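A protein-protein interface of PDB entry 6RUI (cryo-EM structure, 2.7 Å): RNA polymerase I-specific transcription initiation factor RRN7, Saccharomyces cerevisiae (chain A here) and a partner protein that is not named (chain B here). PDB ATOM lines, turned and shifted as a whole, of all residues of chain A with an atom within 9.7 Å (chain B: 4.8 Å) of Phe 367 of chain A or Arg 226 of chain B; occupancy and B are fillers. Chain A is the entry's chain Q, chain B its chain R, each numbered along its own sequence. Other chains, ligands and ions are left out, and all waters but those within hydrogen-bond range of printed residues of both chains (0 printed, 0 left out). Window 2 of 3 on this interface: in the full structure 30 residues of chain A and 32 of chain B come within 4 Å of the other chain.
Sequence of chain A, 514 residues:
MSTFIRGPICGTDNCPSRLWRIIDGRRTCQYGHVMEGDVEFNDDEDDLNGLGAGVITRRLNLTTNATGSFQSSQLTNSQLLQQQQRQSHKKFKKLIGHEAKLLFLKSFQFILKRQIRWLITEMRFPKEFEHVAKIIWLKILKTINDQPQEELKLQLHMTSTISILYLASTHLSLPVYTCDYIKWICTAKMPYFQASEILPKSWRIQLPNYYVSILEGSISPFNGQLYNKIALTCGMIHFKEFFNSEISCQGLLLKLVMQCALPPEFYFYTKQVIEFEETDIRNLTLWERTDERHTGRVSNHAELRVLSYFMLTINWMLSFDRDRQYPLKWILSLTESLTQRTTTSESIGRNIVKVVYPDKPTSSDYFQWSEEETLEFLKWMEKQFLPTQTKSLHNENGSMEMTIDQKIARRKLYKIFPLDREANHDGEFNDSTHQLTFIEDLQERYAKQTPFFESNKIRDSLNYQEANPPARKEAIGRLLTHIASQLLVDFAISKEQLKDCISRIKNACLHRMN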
ATOM      1  N   ARG A 341      16.408  17.501  17.425  1.00  0.00           N
ATOM      2  CA  ARG A 341      16.973  18.128  16.246  1.00  0.00           C
ATOM      3  C   ARG A 341      16.435  19.544  16.138  1.00  0.00           C
ATOM      4  O   ARG A 341      15.219  19.749  16.073  1.00  0.00           O
ATOM      5  CB  ARG A 341      16.607  17.336  14.994  1.00  0.00           C
ATOM      6  CG  ARG A 341      16.911  15.851  15.054  1.00  0.00           C
ATOM      7  CD  ARG A 341      18.389  15.566  15.270  1.00  0.00           C
ATOM      8  NE  ARG A 341      19.235  16.122  14.222  1.00  0.00           N
ATOM      9  CZ  ARG A 341      20.553  16.233  14.322  1.00  0.00           C
ATOM     10  NH1 ARG A 341      21.168  15.804  15.417  1.00  0.00           N
ATOM     11  NH2 ARG A 341      21.256  16.757  13.325  1.00  0.00           N
ATOM     12  N   ASN A 351      26.359  19.719  12.707  1.00  0.00           N
ATOM     13  CA  ASN A 351      25.983  18.651  11.790  1.00  0.00           C
ATOM     14  C   ASN A 351      27.089  18.362  10.794  1.00  0.00           C
ATOM     15  O   ASN A 351      27.244  17.216  10.359  1.00  0.00           O
ATOM     16  CB  ASN A 351      24.712  19.019  11.033  1.00  0.00           C
ATOM     17  CG  ASN A 351      23.486  18.950  11.890  1.00  0.00           C
ATOM     18  OD1 ASN A 351      23.344  18.048  12.712  1.00  0.00           O
ATOM     19  ND2 ASN A 351      22.570  19.883  11.685  1.00  0.00           N
ATOM     20  N   LYS A 354      29.878  15.937  12.143  1.00  0.00           N
ATOM     21  CA  LYS A 354      29.503  14.531  12.109  1.00  0.00           C
ATOM     22  C   LYS A 354      29.702  13.932  10.724  1.00  0.00           C
ATOM     23  O   LYS A 354      29.905  12.720  10.599  1.00  0.00           O
ATOM     24  CB  LYS A 354      28.054  14.384  12.551  1.00  0.00           C
ATOM     25  CG  LYS A 354      27.812  14.797  13.990  1.00  0.00           C
ATOM     26  CD  LYS A 354      26.371  14.531  14.382  1.00  0.00           C
ATOM     27  CE  LYS A 354      26.097  14.868  15.835  1.00  0.00           C
ATOM     28  NZ  LYS A 354      24.679  14.575  16.194  1.00  0.00           N
ATOM     29  N   VAL A 355      29.650  14.767   9.683  1.00  0.00           N
ATOM     30  CA  VAL A 355      29.909  14.318   8.317  1.00  0.00           C
ATOM     31  C   VAL A 355      31.371  13.924   8.140  1.00  0.00           C
ATOM     32  O   VAL A 355      31.678  12.876   7.557  1.00  0.00           O
ATOM     33  CB  VAL A 355      29.494  15.424   7.326  1.00  0.00           C
ATOM     34  CG1 VAL A 355      30.001  15.150   5.931  1.00  0.00           C
ATOM     35  CG2 VAL A 355      27.993  15.612   7.334  1.00  0.00           C
ATOM     36  N   THR A 362      27.149   8.027  15.230  1.00  0.00           N
ATOM     37  CA  THR A 362      26.309   9.157  14.820  1.00  0.00           C
ATOM     38  C   THR A 362      27.063  10.015  13.795  1.00  0.00           C
ATOM     39  O   THR A 362      27.107  11.246  13.863  1.00  0.00           O
ATOM     40  CB  THR A 362      25.819   9.960  16.039  1.00  0.00           C
ATOM     41  OG1 THR A 362      25.447   9.043  17.077  1.00  0.00           O
ATOM     42  CG2 THR A 362      24.557  10.748  15.701  1.00  0.00           C
ATOM     43  N   SER A 363      27.733   9.328  12.875  1.00  0.00           N
ATOM     44  CA  SER A 363      28.240   9.898  11.640  1.00  0.00           C
ATOM     45  C   SER A 363      27.231   9.764  10.515  1.00  0.00           C
ATOM     46  O   SER A 363      27.505  10.193   9.391  1.00  0.00           O
ATOM     47  CB  SER A 363      29.548   9.213  11.250  1.00  0.00           C
ATOM     48  OG  SER A 363      29.340   7.842  10.987  1.00  0.00           O
ATOM     49  N   SER A 364      26.083   9.164  10.810  1.00  0.00           N
ATOM     50  CA  SER A 364      25.007   8.889   9.875  1.00  0.00           C
ATOM     51  C   SER A 364      23.702   9.464  10.398  1.00  0.00           C
ATOM     52  O   SER A 364      22.623   8.912  10.185  1.00  0.00           O
ATOM     53  CB  SER A 364      24.885   7.390   9.630  1.00  0.00           C
ATOM     54  OG  SER A 364      24.556   6.723  10.830  1.00  0.00           O
ATOM     55  N   ASP A 365      23.802  10.591  11.099  1.00  0.00           N
ATOM     56  CA  ASP A 365      22.650  11.308  11.618  1.00  0.00           C
ATOM     57  C   ASP A 365      21.878  12.022  10.517  1.00  0.00           C
ATOM     58  O   ASP A 365      20.712  12.375  10.719  1.00  0.00           O
ATOM     59  CB  ASP A 365      23.121  12.315  12.671  1.00  0.00           C
ATOM     60  CG  ASP A 365      22.021  12.749  13.620  1.00  0.00           C
ATOM     61  OD1 ASP A 365      20.886  12.245  13.523  1.00  0.00           O
ATOM     62  OD2 ASP A 365      22.299  13.604  14.484  1.00  0.00           O
ATOM     63  N   TYR A 366      22.489  12.203   9.344  1.00  0.00           N
ATOM     64  CA  TYR A 366      21.859  12.905   8.235  1.00  0.00           C
ATOM     65  C   TYR A 366      20.665  12.162   7.659  1.00  0.00           C
ATOM     66  O   TYR A 366      19.890  12.770   6.914  1.00  0.00           O
ATOM     67  CB  TYR A 366      22.888  13.184   7.138  1.00  0.00           C
ATOM     68  CG  TYR A 366      23.559  11.959   6.579  1.00  0.00           C
ATOM     69  CD1 TYR A 366      24.737  11.489   7.119  1.00  0.00           C
ATOM     70  CD2 TYR A 366      23.030  11.287   5.493  1.00  0.00           C
ATOM     71  CE1 TYR A 366      25.358  10.374   6.604  1.00  0.00           C
ATOM     72  CE2 TYR A 366      23.632  10.172   4.989  1.00  0.00           C
ATOM     73  CZ  TYR A 366      24.797   9.720   5.540  1.00  0.00           C
ATOM     74  OH  TYR A 366      25.406   8.604   5.026  1.00  0.00           O
ATOM     75  N   PHE A 367      20.505  10.874   7.977  1.00  0.00           N
ATOM     76  CA  PHE A 367      19.273  10.167   7.653  1.00  0.00           C
ATOM     77  C   PHE A 367      18.071  10.760   8.370  1.00  0.00           C
ATOM     78  O   PHE A 367      16.945  10.666   7.874  1.00  0.00           O
ATOM     79  CB  PHE A 367      19.408   8.692   8.014  1.00  0.00           C
ATOM     80  CG  PHE A 367      20.259   7.910   7.065  1.00  0.00           C
ATOM     81  CD1 PHE A 367      19.710   7.368   5.919  1.00  0.00           C
ATOM     82  CD2 PHE A 367      21.604   7.720   7.312  1.00  0.00           C
ATOM     83  CE1 PHE A 367      20.480   6.643   5.045  1.00  0.00           C
ATOM     84  CE2 PHE A 367      22.380   6.997   6.435  1.00  0.00           C
ATOM     85  CZ  PHE A 367      21.815   6.460   5.303  1.00  0.00           C
ATOM     86  N   GLN A 368      18.285  11.381   9.526  1.00  0.00           N
ATOM     87  CA  GLN A 368      17.195  11.862  10.354  1.00  0.00           C
ATOM     88  C   GLN A 368      17.037  13.373  10.294  1.00  0.00           C
ATOM     89  O   GLN A 368      16.391  13.951  11.172  1.00  0.00           O
ATOM     90  CB  GLN A 368      17.392  11.411  11.798  1.00  0.00           C
ATOM     91  CG  GLN A 368      17.270   9.915  12.003  1.00  0.00           C
ATOM     92  CD  GLN A 368      18.566   9.183  11.740  1.00  0.00           C
ATOM     93  OE1 GLN A 368      19.637   9.785  11.748  1.00  0.00           O
ATOM     94  NE2 GLN A 368      18.475   7.886  11.480  1.00  0.00           N
ATOM     95  N   TRP A 369      17.604  14.024   9.286  1.00  0.00           N
ATOM     96  CA  TRP A 369      17.425  15.457   9.144  1.00  0.00           C
ATOM     97  C   TRP A 369      16.031  15.766   8.633  1.00  0.00           C
ATOM     98  O   TRP A 369      15.420  14.978   7.909  1.00  0.00           O
ATOM     99  CB  TRP A 369      18.451  16.054   8.185  1.00  0.00           C
ATOM    100  CG  TRP A 369      19.851  16.062   8.687  1.00  0.00           C
ATOM    101  CD1 TRP A 369      20.285  15.662   9.906  1.00  0.00           C
ATOM    102  CD2 TRP A 369      21.004  16.523   7.981  1.00  0.00           C
ATOM    103  NE1 TRP A 369      21.644  15.826  10.003  1.00  0.00           N
ATOM    104  CE2 TRP A 369      22.107  16.361   8.832  1.00  0.00           C
ATOM    105  CE3 TRP A 369      21.212  17.053   6.709  1.00  0.00           C
ATOM    106  CZ2 TRP A 369      23.396  16.702   8.449  1.00  0.00           C
ATOM    107  CZ3 TRP A 369      22.490  17.390   6.334  1.00  0.00           C
ATOM    108  CH2 TRP A 369      23.565  17.217   7.197  1.00  0.00           C
ATOM    109  N   SER A 370      15.526  16.934   9.010  1.00  0.00           N
ATOM    110  CA  SER A 370      14.221  17.360   8.539  1.00  0.00           C
ATOM    111  C   SER A 370      14.335  17.959   7.147  1.00  0.00           C
ATOM    112  O   SER A 370      15.400  17.968   6.521  1.00  0.00           O
ATOM    113  CB  SER A 370      13.611  18.379   9.493  1.00  0.00           C
ATOM    114  OG  SER A 370      14.283  19.623   9.407  1.00  0.00           O
ATOM    115  N   GLU A 371      13.209  18.472   6.657  1.00  0.00           N
ATOM    116  CA  GLU A 371      13.202  19.223   5.405  1.00  0.00           C
ATOM    117  C   GLU A 371      14.001  20.509   5.536  1.00  0.00           C
ATOM    118  O   GLU A 371      14.855  20.807   4.698  1.00  0.00           O
ATOM    119  CB  GLU A 371      11.766  19.539   5.005  1.00  0.00           C
ATOM    120  CG  GLU A 371      11.618  20.389   3.760  1.00  0.00           C
ATOM    121  CD  GLU A 371      11.923  19.639   2.487  1.00  0.00           C
ATOM    122  OE1 GLU A 371      11.793  18.400   2.485  1.00  0.00           O
ATOM    123  OE2 GLU A 371      12.268  20.291   1.479  1.00  0.00           O
ATOM    124  N   GLU A 373      16.215  21.181   7.740  1.00  0.00           N
ATOM    125  CA  GLU A 373      17.576  20.963   8.203  1.00  0.00           C
ATOM    126  C   GLU A 373      18.529  20.703   7.044  1.00  0.00           C
ATOM    127  O   GLU A 373      19.704  21.078   7.112  1.00  0.00           O
ATOM    128  CB  GLU A 373      17.594  19.819   9.218  1.00  0.00           C
ATOM    129  CG  GLU A 373      18.872  19.709  10.030  1.00  0.00           C
ATOM    130  CD  GLU A 373      18.700  18.827  11.248  1.00  0.00           C
ATOM    131  OE1 GLU A 373      17.613  18.243  11.406  1.00  0.00           O
ATOM    132  OE2 GLU A 373      19.631  18.752  12.075  1.00  0.00           O
ATOM    133  N   THR A 374      18.033  20.110   5.959  1.00  0.00           N
ATOM    134  CA  THR A 374      18.859  19.920   4.774  1.00  0.00           C
ATOM    135  C   THR A 374      19.023  21.221   3.992  1.00  0.00           C
ATOM    136  O   THR A 374      20.072  21.443   3.380  1.00  0.00           O
ATOM    137  CB  THR A 374      18.245  18.820   3.907  1.00  0.00           C
ATOM    138  OG1 THR A 374      18.064  17.649   4.707  1.00  0.00           O
ATOM    139  CG2 THR A 374      19.152  18.432   2.766  1.00  0.00           C
ATOM    140  N   MET B   1      25.116   3.895   2.762  1.00  0.00           N
ATOM    141  CA  MET B   1      24.279   2.826   2.239  1.00  0.00           C
ATOM    142  C   MET B   1      24.337   2.736   0.713  1.00  0.00           C
ATOM    143  O   MET B   1      24.739   1.711   0.172  1.00  0.00           O
ATOM    144  CB  MET B   1      22.837   2.999   2.734  1.00  0.00           C
ATOM    145  CG  MET B   1      21.854   2.025   2.129  1.00  0.00           C
ATOM    146  SD  MET B   1      20.293   1.814   3.013  1.00  0.00           S
ATOM    147  CE  MET B   1      19.541   3.425   2.947  1.00  0.00           C
ATOM    148  N   ASP B 218      23.677   9.578  -0.308  1.00  0.00           N
ATOM    149  CA  ASP B 218      22.705   8.980   0.590  1.00  0.00           C
ATOM    150  C   ASP B 218      21.569   9.936   0.904  1.00  0.00           C
ATOM    151  O   ASP B 218      20.513   9.488   1.336  1.00  0.00           O
ATOM    152  CB  ASP B 218      23.370   8.524   1.883  1.00  0.00           C
ATOM    153  CG  ASP B 218      24.303   7.355   1.681  1.00  0.00           C
ATOM    154  OD1 ASP B 218      24.065   6.553   0.759  1.00  0.00           O
ATOM    155  OD2 ASP B 218      25.278   7.233   2.446  1.00  0.00           O
ATOM    156  N   LEU B 222      17.641   9.311  -0.856  1.00  0.00           N
ATOM    157  CA  LEU B 222      16.691   9.273   0.246  1.00  0.00           C
ATOM    158  C   LEU B 222      15.454  10.096  -0.059  1.00  0.00           C
ATOM    159  O   LEU B 222      14.351   9.744   0.353  1.00  0.00           O
ATOM    160  CB  LEU B 222      17.359   9.792   1.509  1.00  0.00           C
ATOM    161  CG  LEU B 222      16.675   9.645   2.856  1.00  0.00           C
ATOM    162  CD1 LEU B 222      16.555   8.184   3.231  1.00  0.00           C
ATOM    163  CD2 LEU B 222      17.446  10.405   3.914  1.00  0.00           C
ATOM    164  N   ASN B 223      15.618  11.182  -0.787  1.00  0.00           N
ATOM    165  CA  ASN B 223      14.468  11.986  -1.146  1.00  0.00           C
ATOM    166  C   ASN B 223      13.767  11.434  -2.373  1.00  0.00           C
ATOM    167  O   ASN B 223      12.542  11.559  -2.490  1.00  0.00           O
ATOM    168  CB  ASN B 223      14.922  13.420  -1.354  1.00  0.00           C
ATOM    169  CG  ASN B 223      15.340  14.072  -0.063  1.00  0.00           C
ATOM    170  OD1 ASN B 223      14.611  14.045   0.923  1.00  0.00           O
ATOM    171  ND2 ASN B 223      16.545  14.605  -0.039  1.00  0.00           N
ATOM    172  N   VAL B 224      14.520  10.814  -3.284  1.00  0.00           N
ATOM    173  CA  VAL B 224      13.916  10.116  -4.412  1.00  0.00           C
ATOM    174  C   VAL B 224      13.165   8.888  -3.915  1.00  0.00           C
ATOM    175  O   VAL B 224      12.126   8.509  -4.468  1.00  0.00           O
ATOM    176  CB  VAL B 224      15.017   9.779  -5.435  1.00  0.00           C
ATOM    177  CG1 VAL B 224      14.477   9.042  -6.631  1.00  0.00           C
ATOM    178  CG2 VAL B 224      15.666  11.038  -5.889  1.00  0.00           C
ATOM    179  N   SER B 225      13.657   8.276  -2.843  1.00  0.00           N
ATOM    180  CA  SER B 225      12.894   7.263  -2.128  1.00  0.00           C
ATOM    181  C   SER B 225      11.611   7.836  -1.537  1.00  0.00           C
ATOM    182  O   SER B 225      10.564   7.183  -1.561  1.00  0.00           O
ATOM    183  CB  SER B 225      13.769   6.670  -1.031  1.00  0.00           C
ATOM    184  OG  SER B 225      13.020   5.862  -0.172  1.00  0.00           O
ATOM    185  N   ARG B 226      11.667   9.055  -1.013  1.00  0.00           N
ATOM    186  CA  ARG B 226      10.542   9.678  -0.335  1.00  0.00           C
ATOM    187  C   ARG B 226       9.733  10.572  -1.253  1.00  0.00           C
ATOM    188  O   ARG B 226       8.868  11.309  -0.767  1.00  0.00           O
ATOM    189  CB  ARG B 226      11.039  10.484   0.863  1.00  0.00           C
ATOM    190  CG  ARG B 226      11.578   9.643   2.007  1.00  0.00           C
ATOM    191  CD  ARG B 226      12.303  10.539   2.989  1.00  0.00           C
ATOM    192  NE  ARG B 226      13.014   9.796   4.021  1.00  0.00           N
ATOM    193  CZ  ARG B 226      13.878  10.353   4.861  1.00  0.00           C
ATOM    194  NH1 ARG B 226      14.150  11.644   4.768  1.00  0.00           N
ATOM    195  NH2 ARG B 226      14.496   9.615   5.768  1.00  0.00           N
ATOM    196  N   HIS B 227      10.024  10.541  -2.559  1.00  0.00           N
ATOM    197  CA  HIS B 227       9.278  11.251  -3.605  1.00  0.00           C
ATOM    198  C   HIS B 227       9.263  12.756  -3.371  1.00  0.00           C
ATOM    199  O   HIS B 227       8.296  13.445  -3.693  1.00  0.00           O
ATOM    200  CB  HIS B 227       7.858  10.703  -3.745  1.00  0.00           C
ATOM    201  CG  HIS B 227       7.810   9.272  -4.175  1.00  0.00           C
ATOM    202  ND1 HIS B 227       7.828   8.226  -3.281  1.00  0.00           N
ATOM    203  CD2 HIS B 227       7.757   8.712  -5.408  1.00  0.00           C
ATOM    204  CE1 HIS B 227       7.782   7.082  -3.942  1.00  0.00           C
ATOM    205  NE2 HIS B 227       7.740   7.350  -5.234  1.00  0.00           N
ATOM    206  N   ASN B 228      10.346  13.263  -2.797  1.00  0.00           N
ATOM    207  CA  ASN B 228      10.525  14.678  -2.499  1.00  0.00           C
ATOM    208  C   ASN B 228      11.442  15.218  -3.582  1.00  0.00           C
ATOM    209  O   ASN B 228      12.647  14.991  -3.551  1.00  0.00           O
ATOM    210  CB  ASN B 228      11.120  14.866  -1.118  1.00  0.00           C
ATOM    211  CG  ASN B 228      11.111  16.308  -0.669  1.00  0.00           C
ATOM    212  OD1 ASN B 228      10.640  17.194  -1.380  1.00  0.00           O
ATOM    213  ND2 ASN B 228      11.646  16.554   0.516  1.00  0.00           N
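Among the printed residues, pairs that only touch across the chains: Phe 367 of chain A with Met 1 of chain B (3.95 Å).
N of Met 1 of chain B sits at hydrogen-bond distance from OD2 of Asp 218 of chain B (3.4 Å).
The backbone NH of Asn 228 of chain B sits at hydrogen-bond distance from the backbone carbonyl oxygen of Asn 223 of chain B.
Of the 9 printed residues of chain B, 4 touch a printed residue of chain A.
OH of Tyr 366 of chain A sits at hydrogen-bond distance from OD2 of Asp 218 of chain B (2.9 Å).
O of Phe 367 of chain A sits at hydrogen-bond distance from NH2 of Arg 226 of chain B, at 3.4 Å.
The side-chain amide nitrogen (ND2) of Asn 228 of chain B is in hydrogen-bond range of the side-chain carboxylate (OE1) of Glu 371 of chain A (2.7 Å).
Of the printed residues of chain B, Phe 367 of chain A touches Met 1 (3.95 Å) and Arg 226 (3.4 Å).
Arg 226 of chain B touches just one residue of chain A: Phe 367.
No residue of chain A comes within 4 Å of His 227 of chain B.
Of the printed residues of chain B, Glu 371 of chain A touches Asn 228 (2.7 Å).
Printed residues of chain B within 4 Å of Tyr 366 of chain A: Asp 218.
Of the printed residues of chain A, Met 1 of chain B touches Phe 367 (3.95 Å).
Printed residues of chain A within 4 Å of Asn 228 of chain B: Glu 371 (2.7 Å).
The nearest printed residue of chain B that does not touch Phe 367 of chain A is Leu 222 of chain B (4.0001 Å).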
